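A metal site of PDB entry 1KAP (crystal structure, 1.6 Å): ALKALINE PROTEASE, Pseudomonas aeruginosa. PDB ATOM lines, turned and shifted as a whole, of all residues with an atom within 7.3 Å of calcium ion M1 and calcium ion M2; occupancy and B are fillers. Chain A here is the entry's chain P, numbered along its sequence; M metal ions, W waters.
Six residues have an atom within 4 Å of calcium ion M1: Gly 370, Leu 371, Gly 372, Asp 374, Glu 392 and Asp 399.
The nearest printed residue that does not touch calcium ion M1 is Gly 369 (4.1 Å).
Water W1 lies within hydrogen-bond range of OD2 of Asp 399 and N of Gly 370.
Calcium ion M2 is bound by O of Gly 369, O of Leu 371, OD1 of Asp 374, O of Asn 352, O of Val 354 and OD1 of Asn 356.
Slightly farther from calcium ion M2 lies the side-chain carboxylate (OD2) of Asp 374 (3.1 Å).
Calcium ion M1 is bound by OD2 of Asp 374, O of Glu 392, O of Gly 370, water W1, O of Gly 372 and OD1 of Asp 399.
Calcium ion M1 has six donor atoms within binding distance.
OE2 of Glu 392 is in hydrogen-bond range of OH of Tyr 368.
The backbone carbonyl oxygen (O) of Asp 374 is in hydrogen-bond range of the backbone NH (N) of Thr 400 (2.9 Å).
The side-chain hydroxyl (OH) of Tyr 387 is in hydrogen-bond range of the side-chain carboxylate (OD2) of Asp 399, at 2.7 Å.
The side-chain amide nitrogen (ND2) of Asn 352 sits at hydrogen-bond distance from the backbone carbonyl oxygen (O) of Leu 314 (3.0 Å).
OD1 of Asn 352 sits close to N of Val 354, 3.2 Å away.
The side-chain amide nitrogen of Asn 356 is in hydrogen-bond range of the backbone carbonyl oxygen of Glu 338 (2.8 Å).
N of Asp 399 is in hydrogen-bond range of OG of Ser 393, at 2.9 Å.
The backbone carbonyl oxygen (O) of Asn 356 lies within hydrogen-bond range of the backbone NH (N) of Gln 375 (2.9 Å).
Of the 30 residues printed, 7 come within 4 Å of calcium ion M2.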
ATOM      1  N   LEU A 314      20.642  14.389  16.167  1.00  0.00           N
ATOM      2  CA  LEU A 314      20.039  14.322  17.497  1.00  0.00           C
ATOM      3  C   LEU A 314      18.693  15.028  17.681  1.00  0.00           C
ATOM      4  O   LEU A 314      18.155  15.036  18.783  1.00  0.00           O
ATOM      5  CB  LEU A 314      21.015  14.792  18.580  1.00  0.00           C
ATOM      6  CG  LEU A 314      22.307  14.002  18.805  1.00  0.00           C
ATOM      7  CD1 LEU A 314      23.067  14.629  19.973  1.00  0.00           C
ATOM      8  CD2 LEU A 314      22.015  12.519  19.099  1.00  0.00           C
ATOM      9  N   GLU A 338      21.099  13.775  24.392  1.00  0.00           N
ATOM     10  CA  GLU A 338      22.156  14.761  24.535  1.00  0.00           C
ATOM     11  C   GLU A 338      23.473  14.585  23.817  1.00  0.00           C
ATOM     12  O   GLU A 338      24.058  15.558  23.341  1.00  0.00           O
ATOM     13  CB  GLU A 338      22.460  14.966  26.030  1.00  0.00           C
ATOM     14  CG  GLU A 338      21.349  15.601  26.866  1.00  0.00           C
ATOM     15  CD  GLU A 338      20.151  14.693  27.168  1.00  0.00           C
ATOM     16  OE1 GLU A 338      20.225  13.454  26.990  1.00  0.00           O
ATOM     17  OE2 GLU A 338      19.116  15.231  27.604  1.00  0.00           O
ATOM     18  N   ILE A 350      25.140  15.911  13.986  1.00  0.00           N
ATOM     19  CA  ILE A 350      24.305  17.099  14.132  1.00  0.00           C
ATOM     20  C   ILE A 350      23.645  17.091  15.508  1.00  0.00           C
ATOM     21  O   ILE A 350      22.894  16.174  15.851  1.00  0.00           O
ATOM     22  CB  ILE A 350      23.221  17.125  13.022  1.00  0.00           C
ATOM     23  CG1 ILE A 350      23.881  17.224  11.632  1.00  0.00           C
ATOM     24  CG2 ILE A 350      22.221  18.262  13.262  1.00  0.00           C
ATOM     25  CD1 ILE A 350      22.913  17.166  10.478  1.00  0.00           C
ATOM     26  N   GLY A 351      23.978  18.107  16.299  1.00  0.00           N
ATOM     27  CA  GLY A 351      23.409  18.233  17.637  1.00  0.00           C
ATOM     28  C   GLY A 351      22.040  18.888  17.580  1.00  0.00           C
ATOM     29  O   GLY A 351      21.519  19.213  16.507  1.00  0.00           O
ATOM     30  N   ASN A 352      21.433  19.086  18.741  1.00  0.00           N
ATOM     31  CA  ASN A 352      20.129  19.699  18.831  1.00  0.00           C
ATOM     32  C   ASN A 352      20.239  20.994  19.640  1.00  0.00           C
ATOM     33  O   ASN A 352      21.331  21.494  19.844  1.00  0.00           O
ATOM     34  CB  ASN A 352      19.090  18.718  19.412  1.00  0.00           C
ATOM     35  CG  ASN A 352      19.524  18.131  20.728  1.00  0.00           C
ATOM     36  OD1 ASN A 352      20.245  18.745  21.507  1.00  0.00           O
ATOM     37  ND2 ASN A 352      19.101  16.898  20.986  1.00  0.00           N
ATOM     38  N   ASP A 353      19.110  21.515  20.109  1.00  0.00           N
ATOM     39  CA  ASP A 353      19.100  22.786  20.838  1.00  0.00           C
ATOM     40  C   ASP A 353      19.743  22.839  22.210  1.00  0.00           C
ATOM     41  O   ASP A 353      19.943  23.940  22.740  1.00  0.00           O
ATOM     42  CB  ASP A 353      17.672  23.309  20.962  1.00  0.00           C
ATOM     43  CG  ASP A 353      17.031  23.652  19.621  1.00  0.00           C
ATOM     44  OD1 ASP A 353      17.719  23.600  18.569  1.00  0.00           O
ATOM     45  OD2 ASP A 353      15.817  23.989  19.637  1.00  0.00           O
ATOM     46  N   VAL A 354      20.008  21.699  22.833  1.00  0.00           N
ATOM     47  CA  VAL A 354      20.608  21.699  24.159  1.00  0.00           C
ATOM     48  C   VAL A 354      22.115  21.506  24.061  1.00  0.00           C
ATOM     49  O   VAL A 354      22.646  21.299  22.971  1.00  0.00           O
ATOM     50  CB  VAL A 354      19.975  20.609  25.107  1.00  0.00           C
ATOM     51  CG1 VAL A 354      18.455  20.813  25.176  1.00  0.00           C
ATOM     52  CG2 VAL A 354      20.322  19.177  24.655  1.00  0.00           C
ATOM     53  N   ALA A 355      22.806  21.583  25.195  1.00  0.00           N
ATOM     54  CA  ALA A 355      24.249  21.376  25.220  1.00  0.00           C
ATOM     55  C   ALA A 355      24.513  19.893  24.918  1.00  0.00           C
ATOM     56  O   ALA A 355      24.013  19.005  25.630  1.00  0.00           O
ATOM     57  CB  ALA A 355      24.812  21.736  26.582  1.00  0.00           C
ATOM     58  N   ASN A 356      25.260  19.636  23.855  1.00  0.00           N
ATOM     59  CA  ASN A 356      25.572  18.262  23.438  1.00  0.00           C
ATOM     60  C   ASN A 356      27.061  17.975  23.517  1.00  0.00           C
ATOM     61  O   ASN A 356      27.872  18.894  23.362  1.00  0.00           O
ATOM     62  CB  ASN A 356      25.211  18.045  21.959  1.00  0.00           C
ATOM     63  CG  ASN A 356      23.827  18.465  21.635  1.00  0.00           C
ATOM     64  OD1 ASN A 356      23.611  19.332  20.796  1.00  0.00           O
ATOM     65  ND2 ASN A 356      22.850  17.830  22.270  1.00  0.00           N
ATOM     66  N   VAL A 357      27.403  16.712  23.728  1.00  0.00           N
ATOM     67  CA  VAL A 357      28.791  16.274  23.684  1.00  0.00           C
ATOM     68  C   VAL A 357      28.780  15.435  22.401  1.00  0.00           C
ATOM     69  O   VAL A 357      28.009  14.482  22.303  1.00  0.00           O
ATOM     70  CB  VAL A 357      29.218  15.348  24.852  1.00  0.00           C
ATOM     71  CG1 VAL A 357      30.616  14.771  24.595  1.00  0.00           C
ATOM     72  CG2 VAL A 357      29.226  16.124  26.152  1.00  0.00           C
ATOM     73  N   LEU A 358      29.526  15.868  21.388  1.00  0.00           N
ATOM     74  CA  LEU A 358      29.610  15.168  20.113  1.00  0.00           C
ATOM     75  C   LEU A 358      31.076  14.752  19.928  1.00  0.00           C
ATOM     76  O   LEU A 358      31.969  15.587  20.044  1.00  0.00           O
ATOM     77  CB  LEU A 358      29.192  16.071  18.946  1.00  0.00           C
ATOM     78  CG  LEU A 358      27.784  16.664  19.003  1.00  0.00           C
ATOM     79  CD1 LEU A 358      27.561  17.553  17.791  1.00  0.00           C
ATOM     80  CD2 LEU A 358      26.755  15.539  19.041  1.00  0.00           C
ATOM     81  N   TYR A 368      28.287  19.624  13.978  1.00  0.00           N
ATOM     82  CA  TYR A 368      27.444  20.807  14.024  1.00  0.00           C
ATOM     83  C   TYR A 368      26.722  20.796  15.375  1.00  0.00           C
ATOM     84  O   TYR A 368      25.760  20.056  15.561  1.00  0.00           O
ATOM     85  CB  TYR A 368      26.433  20.733  12.895  1.00  0.00           C
ATOM     86  CG  TYR A 368      25.571  21.952  12.748  1.00  0.00           C
ATOM     87  CD1 TYR A 368      25.973  22.998  11.917  1.00  0.00           C
ATOM     88  CD2 TYR A 368      24.336  22.060  13.395  1.00  0.00           C
ATOM     89  CE1 TYR A 368      25.180  24.109  11.715  1.00  0.00           C
ATOM     90  CE2 TYR A 368      23.520  23.172  13.203  1.00  0.00           C
ATOM     91  CZ  TYR A 368      23.954  24.198  12.353  1.00  0.00           C
ATOM     92  OH  TYR A 368      23.168  25.282  12.073  1.00  0.00           O
ATOM     93  N   GLY A 369      27.197  21.595  16.326  1.00  0.00           N
ATOM     94  CA  GLY A 369      26.576  21.595  17.640  1.00  0.00           C
ATOM     95  C   GLY A 369      25.167  22.168  17.743  1.00  0.00           C
ATOM     96  O   GLY A 369      24.394  21.743  18.606  1.00  0.00           O
ATOM     97  N   GLY A 370      24.834  23.119  16.861  1.00  0.00           N
ATOM     98  CA  GLY A 370      23.535  23.763  16.932  1.00  0.00           C
ATOM     99  C   GLY A 370      23.479  24.695  18.145  1.00  0.00           C
ATOM    100  O   GLY A 370      24.522  25.130  18.647  1.00  0.00           O
ATOM    101  N   LEU A 371      22.287  25.009  18.632  1.00  0.00           N
ATOM    102  CA  LEU A 371      22.182  25.879  19.795  1.00  0.00           C
ATOM    103  C   LEU A 371      22.767  25.229  21.044  1.00  0.00           C
ATOM    104  O   LEU A 371      22.981  24.017  21.088  1.00  0.00           O
ATOM    105  CB  LEU A 371      20.720  26.294  20.034  1.00  0.00           C
ATOM    106  CG  LEU A 371      20.006  27.104  18.939  1.00  0.00           C
ATOM    107  CD1 LEU A 371      18.574  27.369  19.353  1.00  0.00           C
ATOM    108  CD2 LEU A 371      20.728  28.422  18.682  1.00  0.00           C
ATOM    109  N   GLY A 372      23.008  26.047  22.073  1.00  0.00           N
ATOM    110  CA  GLY A 372      23.582  25.558  23.305  1.00  0.00           C
ATOM    111  C   GLY A 372      25.105  25.563  23.273  1.00  0.00           C
ATOM    112  O   GLY A 372      25.713  25.696  22.223  1.00  0.00           O
ATOM    113  N   ALA A 373      25.714  25.484  24.444  1.00  0.00           N
ATOM    114  CA  ALA A 373      27.172  25.463  24.562  1.00  0.00           C
ATOM    115  C   ALA A 373      27.608  23.999  24.437  1.00  0.00           C
ATOM    116  O   ALA A 373      27.594  23.234  25.413  1.00  0.00           O
ATOM    117  CB  ALA A 373      27.592  26.012  25.916  1.00  0.00           C
ATOM    118  N   ASP A 374      28.005  23.611  23.231  1.00  0.00           N
ATOM    119  CA  ASP A 374      28.399  22.226  22.986  1.00  0.00           C
ATOM    120  C   ASP A 374      29.871  21.937  23.228  1.00  0.00           C
ATOM    121  O   ASP A 374      30.705  22.826  23.093  1.00  0.00           O
ATOM    122  CB  ASP A 374      27.991  21.861  21.550  1.00  0.00           C
ATOM    123  CG  ASP A 374      26.539  22.217  21.251  1.00  0.00           C
ATOM    124  OD1 ASP A 374      25.637  21.569  21.828  1.00  0.00           O
ATOM    125  OD2 ASP A 374      26.289  23.172  20.504  1.00  0.00           O
ATOM    126  N   GLN A 375      30.160  20.687  23.607  1.00  0.00           N
ATOM    127  CA  GLN A 375      31.527  20.191  23.853  1.00  0.00           C
ATOM    128  C   GLN A 375      31.805  19.328  22.644  1.00  0.00           C
ATOM    129  O   GLN A 375      31.246  18.220  22.527  1.00  0.00           O
ATOM    130  CB  GLN A 375      31.581  19.335  25.108  1.00  0.00           C
ATOM    131  CG  GLN A 375      31.052  20.032  26.336  1.00  0.00           C
ATOM    132  CD  GLN A 375      31.772  21.332  26.585  1.00  0.00           C
ATOM    133  OE1 GLN A 375      32.994  21.339  26.708  1.00  0.00           O
ATOM    134  NE2 GLN A 375      31.044  22.437  26.610  1.00  0.00           N
ATOM    135  N   LEU A 376      32.674  19.802  21.761  1.00  0.00           N
ATOM    136  CA  LEU A 376      32.962  19.117  20.520  1.00  0.00           C
ATOM    137  C   LEU A 376      34.344  18.503  20.432  1.00  0.00           C
ATOM    138  O   LEU A 376      35.352  19.192  20.608  1.00  0.00           O
ATOM    139  CB  LEU A 376      32.710  20.071  19.347  1.00  0.00           C
ATOM    140  CG  LEU A 376      31.359  20.793  19.353  1.00  0.00           C
ATOM    141  CD1 LEU A 376      31.269  21.766  18.193  1.00  0.00           C
ATOM    142  CD2 LEU A 376      30.207  19.769  19.289  1.00  0.00           C
ATOM    143  N   VAL A 386      31.232  23.092  12.145  1.00  0.00           N
ATOM    144  CA  VAL A 386      30.379  23.965  11.368  1.00  0.00           C
ATOM    145  C   VAL A 386      29.388  24.824  12.163  1.00  0.00           C
ATOM    146  O   VAL A 386      28.801  24.373  13.151  1.00  0.00           O
ATOM    147  CB  VAL A 386      29.624  23.121  10.291  1.00  0.00           C
ATOM    148  CG1 VAL A 386      28.744  23.966   9.414  1.00  0.00           C
ATOM    149  CG2 VAL A 386      30.627  22.334   9.440  1.00  0.00           C
ATOM    150  N   TYR A 387      29.218  26.072  11.710  1.00  0.00           N
ATOM    151  CA  TYR A 387      28.307  27.032  12.344  1.00  0.00           C
ATOM    152  C   TYR A 387      27.391  27.657  11.304  1.00  0.00           C
ATOM    153  O   TYR A 387      27.851  28.060  10.238  1.00  0.00           O
ATOM    154  CB  TYR A 387      29.108  28.112  13.067  1.00  0.00           C
ATOM    155  CG  TYR A 387      29.869  27.556  14.231  1.00  0.00           C
ATOM    156  CD1 TYR A 387      31.104  26.932  14.025  1.00  0.00           C
ATOM    157  CD2 TYR A 387      29.302  27.526  15.501  1.00  0.00           C
ATOM    158  CE1 TYR A 387      31.738  26.277  15.066  1.00  0.00           C
ATOM    159  CE2 TYR A 387      29.936  26.888  16.539  1.00  0.00           C
ATOM    160  CZ  TYR A 387      31.150  26.264  16.310  1.00  0.00           C
ATOM    161  OH  TYR A 387      31.762  25.558  17.318  1.00  0.00           O
ATOM    162  N   ALA A 391      23.941  32.625  17.079  1.00  0.00           N
ATOM    163  CA  ALA A 391      23.329  32.128  18.308  1.00  0.00           C
ATOM    164  C   ALA A 391      23.837  30.756  18.738  1.00  0.00           C
ATOM    165  O   ALA A 391      23.729  30.399  19.910  1.00  0.00           O
ATOM    166  CB  ALA A 391      21.814  32.085  18.160  1.00  0.00           C
ATOM    167  N   GLU A 392      24.388  30.012  17.784  1.00  0.00           N
ATOM    168  CA  GLU A 392      24.902  28.688  18.071  1.00  0.00           C
ATOM    169  C   GLU A 392      26.113  28.652  18.984  1.00  0.00           C
ATOM    170  O   GLU A 392      26.404  27.636  19.596  1.00  0.00           O
ATOM    171  CB  GLU A 392      25.161  27.957  16.766  1.00  0.00           C
ATOM    172  CG  GLU A 392      23.869  27.694  16.038  1.00  0.00           C
ATOM    173  CD  GLU A 392      24.076  27.141  14.667  1.00  0.00           C
ATOM    174  OE1 GLU A 392      25.227  26.934  14.248  1.00  0.00           O
ATOM    175  OE2 GLU A 392      23.062  26.919  13.986  1.00  0.00           O
ATOM    176  N   SER A 393      26.843  29.773  19.078  1.00  0.00           N
ATOM    177  CA  SER A 393      27.991  29.830  19.975  1.00  0.00           C
ATOM    178  C   SER A 393      28.129  31.294  20.366  1.00  0.00           C
ATOM    179  O   SER A 393      29.032  31.993  19.921  1.00  0.00           O
ATOM    180  CB  SER A 393      29.254  29.323  19.275  1.00  0.00           C
ATOM    181  OG  SER A 393      30.243  29.003  20.254  1.00  0.00           O
ATOM    182  N   SER A 394      27.176  31.760  21.166  1.00  0.00           N
ATOM    183  CA  SER A 394      27.167  33.147  21.608  1.00  0.00           C
ATOM    184  C   SER A 394      28.273  33.370  22.630  1.00  0.00           C
ATOM    185  O   SER A 394      28.732  32.435  23.293  1.00  0.00           O
ATOM    186  CB  SER A 394      25.815  33.485  22.231  1.00  0.00           C
ATOM    187  OG  SER A 394      25.647  32.778  23.446  1.00  0.00           O
ATOM    188  N   ALA A 397      27.477  31.810  25.999  1.00  0.00           N
ATOM    189  CA  ALA A 397      27.502  30.361  26.185  1.00  0.00           C
ATOM    190  C   ALA A 397      28.208  29.760  24.960  1.00  0.00           C
ATOM    191  O   ALA A 397      27.562  29.187  24.070  1.00  0.00           O
ATOM    192  CB  ALA A 397      26.087  29.816  26.313  1.00  0.00           C
ATOM    193  N   PRO A 398      29.529  29.900  24.904  1.00  0.00           N
ATOM    194  CA  PRO A 398      30.274  29.366  23.764  1.00  0.00           C
ATOM    195  C   PRO A 398      30.534  27.868  23.783  1.00  0.00           C
ATOM    196  O   PRO A 398      30.582  27.236  24.840  1.00  0.00           O
ATOM    197  CB  PRO A 398      31.595  30.135  23.830  1.00  0.00           C
ATOM    198  CG  PRO A 398      31.812  30.284  25.309  1.00  0.00           C
ATOM    199  CD  PRO A 398      30.431  30.622  25.834  1.00  0.00           C
ATOM    200  N   ASP A 399      30.687  27.308  22.593  1.00  0.00           N
ATOM    201  CA  ASP A 399      31.040  25.908  22.461  1.00  0.00           C
ATOM    202  C   ASP A 399      32.504  25.828  22.913  1.00  0.00           C
ATOM    203  O   ASP A 399      33.201  26.847  22.984  1.00  0.00           O
ATOM    204  CB  ASP A 399      31.099  25.507  20.989  1.00  0.00           C
ATOM    205  CG  ASP A 399      29.745  25.360  20.320  1.00  0.00           C
ATOM    206  OD1 ASP A 399      28.681  25.455  20.965  1.00  0.00           O
ATOM    207  OD2 ASP A 399      29.789  25.129  19.096  1.00  0.00           O
ATOM    208  N   THR A 400      32.969  24.618  23.140  1.00  0.00           N
ATOM    209  CA  THR A 400      34.376  24.389  23.439  1.00  0.00           C
ATOM    210  C   THR A 400      34.807  23.266  22.491  1.00  0.00           C
ATOM    211  O   THR A 400      34.161  22.216  22.451  1.00  0.00           O
ATOM    212  CB  THR A 400      34.633  23.960  24.884  1.00  0.00           C
ATOM    213  OG1 THR A 400      34.247  25.014  25.771  1.00  0.00           O
ATOM    214  CG2 THR A 400      36.122  23.674  25.084  1.00  0.00           C
HETATM  215 CA    CA M   1      26.477  25.343  19.972  1.00  0.00          CA
HETATM  216 CA    CA M   2      23.521  21.750  20.768  1.00  0.00          CA
HETATM  217  O   HOH W   1      27.491  24.875  17.853  1.00  0.00           O
